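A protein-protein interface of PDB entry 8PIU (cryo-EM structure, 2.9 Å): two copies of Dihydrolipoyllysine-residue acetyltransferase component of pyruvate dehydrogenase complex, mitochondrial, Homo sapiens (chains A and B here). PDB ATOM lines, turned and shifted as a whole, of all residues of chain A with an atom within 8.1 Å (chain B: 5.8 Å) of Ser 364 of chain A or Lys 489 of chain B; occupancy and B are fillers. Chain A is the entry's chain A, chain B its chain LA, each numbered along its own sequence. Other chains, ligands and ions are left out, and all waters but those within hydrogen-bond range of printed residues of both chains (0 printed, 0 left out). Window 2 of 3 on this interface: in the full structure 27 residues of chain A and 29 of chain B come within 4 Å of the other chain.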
ATOM      1  N   TYR A 361       4.937 -13.113 -29.329  1.00  0.00           N
ATOM      2  CA  TYR A 361       5.697 -12.444 -28.282  1.00  0.00           C
ATOM      3  C   TYR A 361       5.012 -11.126 -27.957  1.00  0.00           C
ATOM      4  O   TYR A 361       4.489 -10.456 -28.846  1.00  0.00           O
ATOM      5  CB  TYR A 361       7.165 -12.236 -28.677  1.00  0.00           C
ATOM      6  CG  TYR A 361       7.411 -11.114 -29.643  1.00  0.00           C
ATOM      7  CD1 TYR A 361       7.289 -11.313 -31.006  1.00  0.00           C
ATOM      8  CD2 TYR A 361       7.785  -9.857 -29.194  1.00  0.00           C
ATOM      9  CE1 TYR A 361       7.518 -10.292 -31.895  1.00  0.00           C
ATOM     10  CE2 TYR A 361       8.014  -8.829 -30.075  1.00  0.00           C
ATOM     11  CZ  TYR A 361       7.877  -9.053 -31.426  1.00  0.00           C
ATOM     12  OH  TYR A 361       8.103  -8.034 -32.314  1.00  0.00           O
ATOM     13  N   TYR A 362       5.024 -10.762 -26.683  1.00  0.00           N
ATOM     14  CA  TYR A 362       4.150  -9.729 -26.150  1.00  0.00           C
ATOM     15  C   TYR A 362       4.955  -8.503 -25.747  1.00  0.00           C
ATOM     16  O   TYR A 362       6.024  -8.627 -25.152  1.00  0.00           O
ATOM     17  CB  TYR A 362       3.367 -10.274 -24.954  1.00  0.00           C
ATOM     18  CG  TYR A 362       2.827 -11.662 -25.208  1.00  0.00           C
ATOM     19  CD1 TYR A 362       1.634 -11.848 -25.885  1.00  0.00           C
ATOM     20  CD2 TYR A 362       3.524 -12.788 -24.793  1.00  0.00           C
ATOM     21  CE1 TYR A 362       1.145 -13.106 -26.132  1.00  0.00           C
ATOM     22  CE2 TYR A 362       3.041 -14.053 -25.039  1.00  0.00           C
ATOM     23  CZ  TYR A 362       1.851 -14.205 -25.709  1.00  0.00           C
ATOM     24  OH  TYR A 362       1.359 -15.462 -25.956  1.00  0.00           O
ATOM     25  N   LEU A 363       4.438  -7.321 -26.086  1.00  0.00           N
ATOM     26  CA  LEU A 363       5.063  -6.047 -25.749  1.00  0.00           C
ATOM     27  C   LEU A 363       4.018  -5.154 -25.102  1.00  0.00           C
ATOM     28  O   LEU A 363       2.963  -4.920 -25.688  1.00  0.00           O
ATOM     29  CB  LEU A 363       5.631  -5.365 -26.996  1.00  0.00           C
ATOM     30  CG  LEU A 363       6.743  -6.039 -27.793  1.00  0.00           C
ATOM     31  CD1 LEU A 363       6.532  -5.785 -29.264  1.00  0.00           C
ATOM     32  CD2 LEU A 363       8.085  -5.502 -27.360  1.00  0.00           C
ATOM     33  N   SER A 364       4.315  -4.624 -23.924  1.00  0.00           N
ATOM     34  CA  SER A 364       3.334  -3.866 -23.160  1.00  0.00           C
ATOM     35  C   SER A 364       3.814  -2.442 -22.927  1.00  0.00           C
ATOM     36  O   SER A 364       4.982  -2.218 -22.604  1.00  0.00           O
ATOM     37  CB  SER A 364       3.048  -4.540 -21.818  1.00  0.00           C
ATOM     38  OG  SER A 364       2.147  -3.771 -21.043  1.00  0.00           O
ATOM     39  N   ILE A 365       2.906  -1.476 -23.097  1.00  0.00           N
ATOM     40  CA  ILE A 365       3.175  -0.081 -22.759  1.00  0.00           C
ATOM     41  C   ILE A 365       1.966   0.501 -22.039  1.00  0.00           C
ATOM     42  O   ILE A 365       0.916  -0.132 -21.912  1.00  0.00           O
ATOM     43  CB  ILE A 365       3.524   0.794 -23.986  1.00  0.00           C
ATOM     44  CG1 ILE A 365       2.305   0.975 -24.892  1.00  0.00           C
ATOM     45  CG2 ILE A 365       4.697   0.224 -24.762  1.00  0.00           C
ATOM     46  CD1 ILE A 365       2.427   2.132 -25.847  1.00  0.00           C
ATOM     47  N   ASP A 366       2.134   1.734 -21.568  1.00  0.00           N
ATOM     48  CA  ASP A 366       1.121   2.465 -20.822  1.00  0.00           C
ATOM     49  C   ASP A 366       0.902   3.826 -21.472  1.00  0.00           C
ATOM     50  O   ASP A 366       1.855   4.465 -21.928  1.00  0.00           O
ATOM     51  CB  ASP A 366       1.542   2.622 -19.359  1.00  0.00           C
ATOM     52  CG  ASP A 366       0.414   3.091 -18.472  1.00  0.00           C
ATOM     53  OD1 ASP A 366      -0.189   4.139 -18.777  1.00  0.00           O
ATOM     54  OD2 ASP A 366       0.129   2.411 -17.463  1.00  0.00           O
ATOM     55  N   VAL A 367      -0.354   4.266 -21.508  1.00  0.00           N
ATOM     56  CA  VAL A 367      -0.778   5.450 -22.246  1.00  0.00           C
ATOM     57  C   VAL A 367      -1.570   6.350 -21.310  1.00  0.00           C
ATOM     58  O   VAL A 367      -2.443   5.875 -20.576  1.00  0.00           O
ATOM     59  CB  VAL A 367      -1.629   5.071 -23.473  1.00  0.00           C
ATOM     60  CG1 VAL A 367      -1.956   6.304 -24.298  1.00  0.00           C
ATOM     61  CG2 VAL A 367      -0.921   4.030 -24.319  1.00  0.00           C
ATOM     62  N   LYS A 489      -6.919  -5.401 -16.106  1.00  0.00           N
ATOM     63  CA  LYS A 489      -5.806  -4.462 -16.143  1.00  0.00           C
ATOM     64  C   LYS A 489      -4.883  -4.728 -17.326  1.00  0.00           C
ATOM     65  O   LYS A 489      -4.490  -3.797 -18.035  1.00  0.00           O
ATOM     66  CB  LYS A 489      -5.024  -4.538 -14.832  1.00  0.00           C
ATOM     67  CG  LYS A 489      -4.086  -3.378 -14.605  1.00  0.00           C
ATOM     68  CD  LYS A 489      -3.344  -3.530 -13.297  1.00  0.00           C
ATOM     69  CE  LYS A 489      -2.562  -2.276 -12.966  1.00  0.00           C
ATOM     70  NZ  LYS A 489      -3.461  -1.104 -12.821  1.00  0.00           N
ATOM     71  N   ASN A 490      -4.534  -5.990 -17.548  1.00  0.00           N
ATOM     72  CA  ASN A 490      -3.698  -6.395 -18.664  1.00  0.00           C
ATOM     73  C   ASN A 490      -4.163  -7.757 -19.140  1.00  0.00           C
ATOM     74  O   ASN A 490      -4.693  -8.548 -18.361  1.00  0.00           O
ATOM     75  CB  ASN A 490      -2.214  -6.470 -18.277  1.00  0.00           C
ATOM     76  CG  ASN A 490      -1.520  -5.127 -18.344  1.00  0.00           C
ATOM     77  OD1 ASN A 490      -1.172  -4.648 -19.426  1.00  0.00           O
ATOM     78  ND2 ASN A 490      -1.297  -4.516 -17.185  1.00  0.00           N
ATOM     79  N   PHE A 491      -3.965  -8.025 -20.425  1.00  0.00           N
ATOM     80  CA  PHE A 491      -4.157  -9.374 -20.930  1.00  0.00           C
ATOM     81  C   PHE A 491      -3.431  -9.514 -22.258  1.00  0.00           C
ATOM     82  O   PHE A 491      -3.112  -8.526 -22.922  1.00  0.00           O
ATOM     83  CB  PHE A 491      -5.644  -9.740 -21.055  1.00  0.00           C
ATOM     84  CG  PHE A 491      -6.379  -9.017 -22.142  1.00  0.00           C
ATOM     85  CD1 PHE A 491      -6.768  -7.701 -21.979  1.00  0.00           C
ATOM     86  CD2 PHE A 491      -6.723  -9.672 -23.307  1.00  0.00           C
ATOM     87  CE1 PHE A 491      -7.455  -7.049 -22.967  1.00  0.00           C
ATOM     88  CE2 PHE A 491      -7.409  -9.020 -24.297  1.00  0.00           C
ATOM     89  CZ  PHE A 491      -7.779  -7.708 -24.126  1.00  0.00           C
ATOM     90  N   SER A 492      -3.163 -10.763 -22.623  1.00  0.00           N
ATOM     91  CA  SER A 492      -2.387 -11.105 -23.809  1.00  0.00           C
ATOM     92  C   SER A 492      -3.243 -12.002 -24.691  1.00  0.00           C
ATOM     93  O   SER A 492      -3.491 -13.162 -24.347  1.00  0.00           O
ATOM     94  CB  SER A 492      -1.082 -11.794 -23.421  1.00  0.00           C
ATOM     95  OG  SER A 492      -0.369 -11.026 -22.469  1.00  0.00           O
ATOM     96  N   LEU A 503      -3.926  -6.096 -30.871  1.00  0.00           N
ATOM     97  CA  LEU A 503      -3.810  -5.167 -29.758  1.00  0.00           C
ATOM     98  C   LEU A 503      -4.826  -5.529 -28.685  1.00  0.00           C
ATOM     99  O   LEU A 503      -5.959  -5.905 -28.993  1.00  0.00           O
ATOM    100  CB  LEU A 503      -4.018  -3.727 -30.227  1.00  0.00           C
ATOM    101  CG  LEU A 503      -3.750  -2.616 -29.213  1.00  0.00           C
ATOM    102  CD1 LEU A 503      -2.294  -2.605 -28.782  1.00  0.00           C
ATOM    103  CD2 LEU A 503      -4.146  -1.272 -29.787  1.00  0.00           C
ATOM    104  N   ALA A 504      -4.403  -5.439 -27.428  1.00  0.00           N
ATOM    105  CA  ALA A 504      -5.235  -5.780 -26.282  1.00  0.00           C
ATOM    106  C   ALA A 504      -5.286  -4.581 -25.348  1.00  0.00           C
ATOM    107  O   ALA A 504      -4.247  -4.123 -24.867  1.00  0.00           O
ATOM    108  CB  ALA A 504      -4.686  -7.007 -25.558  1.00  0.00           C
ATOM    109  N   MET A 527      -3.811   3.793 -19.082  1.00  0.00           N
ATOM    110  CA  MET A 527      -4.354   2.609 -19.725  1.00  0.00           C
ATOM    111  C   MET A 527      -3.208   1.769 -20.262  1.00  0.00           C
ATOM    112  O   MET A 527      -2.296   2.284 -20.905  1.00  0.00           O
ATOM    113  CB  MET A 527      -5.308   2.999 -20.857  1.00  0.00           C
ATOM    114  CG  MET A 527      -5.954   1.843 -21.574  1.00  0.00           C
ATOM    115  SD  MET A 527      -6.779   2.406 -23.065  1.00  0.00           S
ATOM    116  CE  MET A 527      -5.371   2.907 -24.049  1.00  0.00           C
ATOM    117  N   SER A 528      -3.258   0.468 -20.013  1.00  0.00           N
ATOM    118  CA  SER A 528      -2.169  -0.427 -20.375  1.00  0.00           C
ATOM    119  C   SER A 528      -2.573  -1.250 -21.586  1.00  0.00           C
ATOM    120  O   SER A 528      -3.667  -1.819 -21.615  1.00  0.00           O
ATOM    121  CB  SER A 528      -1.794  -1.339 -19.208  1.00  0.00           C
ATOM    122  OG  SER A 528      -2.923  -2.054 -18.746  1.00  0.00           O
ATOM    123  N   VAL A 529      -1.695  -1.305 -22.586  1.00  0.00           N
ATOM    124  CA  VAL A 529      -1.975  -2.019 -23.826  1.00  0.00           C
ATOM    125  C   VAL A 529      -0.845  -2.997 -24.109  1.00  0.00           C
ATOM    126  O   VAL A 529       0.334  -2.686 -23.903  1.00  0.00           O
ATOM    127  CB  VAL A 529      -2.183  -1.055 -25.016  1.00  0.00           C
ATOM    128  CG1 VAL A 529      -3.472  -0.281 -24.845  1.00  0.00           C
ATOM    129  CG2 VAL A 529      -1.025  -0.102 -25.145  1.00  0.00           C
ATOM    130  N   THR A 530      -1.213  -4.190 -24.569  1.00  0.00           N
ATOM    131  CA  THR A 530      -0.267  -5.235 -24.930  1.00  0.00           C
ATOM    132  C   THR A 530      -0.465  -5.586 -26.395  1.00  0.00           C
ATOM    133  O   THR A 530      -1.580  -5.896 -26.818  1.00  0.00           O
ATOM    134  CB  THR A 530      -0.442  -6.487 -24.057  1.00  0.00           C
ATOM    135  OG1 THR A 530      -0.038  -6.202 -22.714  1.00  0.00           O
ATOM    136  CG2 THR A 530       0.392  -7.641 -24.586  1.00  0.00           C
ATOM    137  N   LEU A 531       0.618  -5.541 -27.156  1.00  0.00           N
ATOM    138  CA  LEU A 531       0.639  -5.952 -28.549  1.00  0.00           C
ATOM    139  C   LEU A 531       1.262  -7.339 -28.628  1.00  0.00           C
ATOM    140  O   LEU A 531       2.363  -7.556 -28.116  1.00  0.00           O
ATOM    141  CB  LEU A 531       1.429  -4.946 -29.385  1.00  0.00           C
ATOM    142  CG  LEU A 531       1.428  -5.057 -30.907  1.00  0.00           C
ATOM    143  CD1 LEU A 531       0.064  -4.722 -31.471  1.00  0.00           C
ATOM    144  CD2 LEU A 531       2.485  -4.139 -31.484  1.00  0.00           C
ATOM    145  N   SER A 532       0.553  -8.274 -29.246  1.00  0.00           N
ATOM    146  CA  SER A 532       1.038  -9.640 -29.429  1.00  0.00           C
ATOM    147  C   SER A 532       1.496  -9.770 -30.875  1.00  0.00           C
ATOM    148  O   SER A 532       0.676  -9.869 -31.788  1.00  0.00           O
ATOM    149  CB  SER A 532      -0.047 -10.656 -29.096  1.00  0.00           C
ATOM    150  OG  SER A 532      -0.597 -10.421 -27.812  1.00  0.00           O
ATOM    151  N   GLY A 543       7.945  -3.599 -33.373  1.00  0.00           N
ATOM    152  CA  GLY A 543       6.770  -3.517 -32.522  1.00  0.00           C
ATOM    153  C   GLY A 543       6.856  -2.382 -31.521  1.00  0.00           C
ATOM    154  O   GLY A 543       5.854  -1.728 -31.215  1.00  0.00           O
ATOM    155  N   LEU A 547       4.277   0.759 -31.124  1.00  0.00           N
ATOM    156  CA  LEU A 547       3.671   1.171 -29.862  1.00  0.00           C
ATOM    157  C   LEU A 547       3.988   2.626 -29.539  1.00  0.00           C
ATOM    158  O   LEU A 547       3.140   3.344 -29.001  1.00  0.00           O
ATOM    159  CB  LEU A 547       4.136   0.254 -28.734  1.00  0.00           C
ATOM    160  CG  LEU A 547       3.504  -1.137 -28.682  1.00  0.00           C
ATOM    161  CD1 LEU A 547       4.312  -2.047 -27.788  1.00  0.00           C
ATOM    162  CD2 LEU A 547       2.073  -1.050 -28.187  1.00  0.00           C
ATOM    163  N   GLY B 487      10.916   2.900 -25.001  1.00  0.00           N
ATOM    164  CA  GLY B 487       9.804   3.182 -24.123  1.00  0.00           C
ATOM    165  C   GLY B 487       8.995   1.978 -23.707  1.00  0.00           C
ATOM    166  O   GLY B 487       7.985   2.145 -23.014  1.00  0.00           O
ATOM    167  N   ILE B 488       9.401   0.771 -24.109  1.00  0.00           N
ATOM    168  CA  ILE B 488       8.682  -0.433 -23.717  1.00  0.00           C
ATOM    169  C   ILE B 488       8.759  -0.601 -22.209  1.00  0.00           C
ATOM    170  O   ILE B 488       9.831  -0.482 -21.607  1.00  0.00           O
ATOM    171  CB  ILE B 488       9.259  -1.653 -24.447  1.00  0.00           C
ATOM    172  CG1 ILE B 488       9.043  -1.517 -25.950  1.00  0.00           C
ATOM    173  CG2 ILE B 488       8.623  -2.930 -23.947  1.00  0.00           C
ATOM    174  CD1 ILE B 488       7.598  -1.399 -26.338  1.00  0.00           C
ATOM    175  N   LYS B 489       7.611  -0.873 -21.590  1.00  0.00           N
ATOM    176  CA  LYS B 489       7.537  -1.067 -20.148  1.00  0.00           C
ATOM    177  C   LYS B 489       7.799  -2.518 -19.760  1.00  0.00           C
ATOM    178  O   LYS B 489       8.563  -2.789 -18.830  1.00  0.00           O
ATOM    179  CB  LYS B 489       6.167  -0.619 -19.638  1.00  0.00           C
ATOM    180  CG  LYS B 489       6.098  -0.431 -18.143  1.00  0.00           C
ATOM    181  CD  LYS B 489       4.714   0.002 -17.716  1.00  0.00           C
ATOM    182  CE  LYS B 489       4.693   0.391 -16.253  1.00  0.00           C
ATOM    183  NZ  LYS B 489       5.604   1.531 -15.985  1.00  0.00           N
ATOM    184  N   ASN B 490       7.172  -3.453 -20.466  1.00  0.00           N
ATOM    185  CA  ASN B 490       7.361  -4.875 -20.237  1.00  0.00           C
ATOM    186  C   ASN B 490       7.276  -5.589 -21.571  1.00  0.00           C
ATOM    187  O   ASN B 490       6.598  -5.128 -22.490  1.00  0.00           O
ATOM    188  CB  ASN B 490       6.307  -5.451 -19.283  1.00  0.00           C
ATOM    189  CG  ASN B 490       6.659  -5.248 -17.825  1.00  0.00           C
ATOM    190  OD1 ASN B 490       7.494  -5.966 -17.271  1.00  0.00           O
ATOM    191  ND2 ASN B 490       6.009  -4.280 -17.188  1.00  0.00           N
ATOM    192  N   PHE B 491       7.972  -6.715 -21.676  1.00  0.00           N
ATOM    193  CA  PHE B 491       7.777  -7.592 -22.819  1.00  0.00           C
ATOM    194  C   PHE B 491       8.302  -8.976 -22.475  1.00  0.00           C
ATOM    195  O   PHE B 491       9.098  -9.149 -21.550  1.00  0.00           O
ATOM    196  CB  PHE B 491       8.432  -7.037 -24.093  1.00  0.00           C
ATOM    197  CG  PHE B 491       9.929  -7.053 -24.087  1.00  0.00           C
ATOM    198  CD1 PHE B 491      10.644  -6.111 -23.371  1.00  0.00           C
ATOM    199  CD2 PHE B 491      10.622  -7.981 -24.839  1.00  0.00           C
ATOM    200  CE1 PHE B 491      12.013  -6.117 -23.380  1.00  0.00           C
ATOM    201  CE2 PHE B 491      11.991  -7.988 -24.850  1.00  0.00           C
ATOM    202  CZ  PHE B 491      12.687  -7.054 -24.122  1.00  0.00           C
ATOM    203  N   ILE B 505      14.489  -6.726 -20.608  1.00  0.00           N
ATOM    204  CA  ILE B 505      14.623  -5.505 -19.824  1.00  0.00           C
ATOM    205  C   ILE B 505      13.821  -4.403 -20.500  1.00  0.00           C
ATOM    206  O   ILE B 505      13.942  -4.189 -21.712  1.00  0.00           O
ATOM    207  CB  ILE B 505      16.098  -5.095 -19.655  1.00  0.00           C
ATOM    208  CG1 ILE B 505      16.846  -6.098 -18.781  1.00  0.00           C
ATOM    209  CG2 ILE B 505      16.204  -3.726 -19.031  1.00  0.00           C
ATOM    210  CD1 ILE B 505      17.482  -7.221 -19.546  1.00  0.00           C
ATOM    211  N   GLY B 506      12.984  -3.723 -19.716  1.00  0.00           N
ATOM    212  CA  GLY B 506      12.185  -2.622 -20.199  1.00  0.00           C
ATOM    213  C   GLY B 506      12.698  -1.279 -19.713  1.00  0.00           C
ATOM    214  O   GLY B 506      13.768  -1.161 -19.112  1.00  0.00           O
ATOM    215  N   ALA B 507      11.905  -0.247 -19.980  1.00  0.00           N
ATOM    216  CA  ALA B 507      12.319   1.114 -19.680  1.00  0.00           C
ATOM    217  C   ALA B 507      12.375   1.359 -18.177  1.00  0.00           C
ATOM    218  O   ALA B 507      11.642   0.750 -17.394  1.00  0.00           O
ATOM    219  CB  ALA B 507      11.371   2.115 -20.332  1.00  0.00           C
ATOM    220  N   GLU B 509      11.679   3.993 -15.237  1.00  0.00           N
ATOM    221  CA  GLU B 509      10.728   5.076 -15.048  1.00  0.00           C
ATOM    222  C   GLU B 509      10.720   5.512 -13.591  1.00  0.00           C
ATOM    223  O   GLU B 509      10.943   4.706 -12.686  1.00  0.00           O
ATOM    224  CB  GLU B 509       9.319   4.650 -15.472  1.00  0.00           C
ATOM    225  CG  GLU B 509       9.229   4.178 -16.912  1.00  0.00           C
ATOM    226  CD  GLU B 509       7.987   3.357 -17.187  1.00  0.00           C
ATOM    227  OE1 GLU B 509       7.056   3.388 -16.356  1.00  0.00           O
ATOM    228  OE2 GLU B 509       7.947   2.676 -18.233  1.00  0.00           O
ATOM    229  N   LYS B 511       8.928   6.178 -10.518  1.00  0.00           N
ATOM    230  CA  LYS B 511       7.676   5.880  -9.846  1.00  0.00           C
ATOM    231  C   LYS B 511       7.562   6.703  -8.566  1.00  0.00           C
ATOM    232  O   LYS B 511       8.428   7.513  -8.235  1.00  0.00           O
ATOM    233  CB  LYS B 511       7.572   4.386  -9.557  1.00  0.00           C
ATOM    234  CG  LYS B 511       7.531   3.531 -10.804  1.00  0.00           C
ATOM    235  CD  LYS B 511       6.402   3.970 -11.712  1.00  0.00           C
ATOM    236  CE  LYS B 511       6.365   3.160 -12.992  1.00  0.00           C
ATOM    237  NZ  LYS B 511       5.285   3.638 -13.899  1.00  0.00           N
ATOM    238  N   SER B 528      11.434  -2.839 -14.910  1.00  0.00           N
ATOM    239  CA  SER B 528      10.717  -4.105 -14.850  1.00  0.00           C
ATOM    240  C   SER B 528      11.392  -5.109 -15.767  1.00  0.00           C
ATOM    241  O   SER B 528      11.683  -4.798 -16.926  1.00  0.00           O
ATOM    242  CB  SER B 528       9.250  -3.925 -15.236  1.00  0.00           C
ATOM    243  OG  SER B 528       9.134  -3.322 -16.509  1.00  0.00           O
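O of Ser 364 of chain A lies within hydrogen-bond range of N of Lys 489 of chain B (3.1 Å).
O of Asn 490 of chain B sits at hydrogen-bond distance from N of Ser 364 of chain A (2.7 Å).
The backbone NH (N) of Leu 531 of chain A lies within hydrogen-bond range of the backbone carbonyl oxygen (O) of Leu 363 of chain A, 2.8 Å away.
The backbone NH (N) of Val 529 of chain A is in hydrogen-bond range of the backbone carbonyl oxygen (O) of Ile 365 of chain A (2.9 Å).
The backbone NH (N) of Ala 507 of chain B sits at hydrogen-bond distance from the backbone carbonyl oxygen (O) of Ile 488 of chain B.
The side-chain amino group (NZ) of Lys 489 of chain B is in salt-bridge range of the side-chain carboxylate (OE2) of Glu 509 of chain B (3.4 Å).
O of Lys 489 of chain B lies within hydrogen-bond range of OG of Ser 528 of chain B (2.4 Å).
The side-chain hydroxyl (OG) of Ser 528 of chain B is in hydrogen-bond range of the side-chain amide oxygen (OD1) of Asn 490 of chain B (3.2 Å).
O of Tyr 362 of chain A touches CB of Phe 491 of chain B (3.1 Å).
O of Asn 490 of chain B touches C of Leu 363 of chain A (3.7 Å).
Leu 363 of chain A touches Phe 491 of chain B (CD2 to CB, 3.6 Å).
Ser 364 of chain A touches Ile 488 of chain B (O to CG2, 3.9 Å).
Ile 488 of chain B touches Ile 365 of chain A.
Leu 547 of chain A touches Ile 488 of chain B (CD1 to CD1, 3.6 Å).
Of the printed residues of chain B, Leu 363 of chain A touches Asn 490 and Phe 491.
Ser 364 of chain A touches three residues of chain B.
Asn 490 of chain A touches none of the printed residues of chain B.
Gly 543 of chain A touches none of the printed residues of chain B.
Printed residues of chain B within 4 Å of Leu 547 of chain A: Ile 488 (3.6 Å).
Of the printed residues of chain A, Ile 488 of chain B touches Ser 364, Ile 365 and Leu 547.
Lys 489 of chain B touches just one residue of chain A: Ser 364 (3.1 Å).
Asn 490 of chain B touches just these residues of chain A: Leu 363 and Ser 364.
Of the printed residues of chain A, Phe 491 of chain B touches Tyr 362 (3.1 Å) and Leu 363 (3.6 Å).
The nearest residue of chain B that does not touch Ser 364 of chain A is Phe 491 of chain B (4.7 Å).
The nearest residue of chain A that does not touch Lys 489 of chain B is Ile 365 of chain A (4.4 Å).
Of the 11 printed residues of chain B, 4 touch a printed residue of chain A.
Hydrophobic or aromatic side chains of chain B that line the printed part of chain A: Ile 488 and Phe 491.
Hydrophobic or aromatic side chains of chain A that line the printed part of chain B: Leu 363, Ile 365 and Leu 547.
Among the printed residues, 8 pairs touch across the chains.
Positions printed for both chains: 489, 490, 491 and 528.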
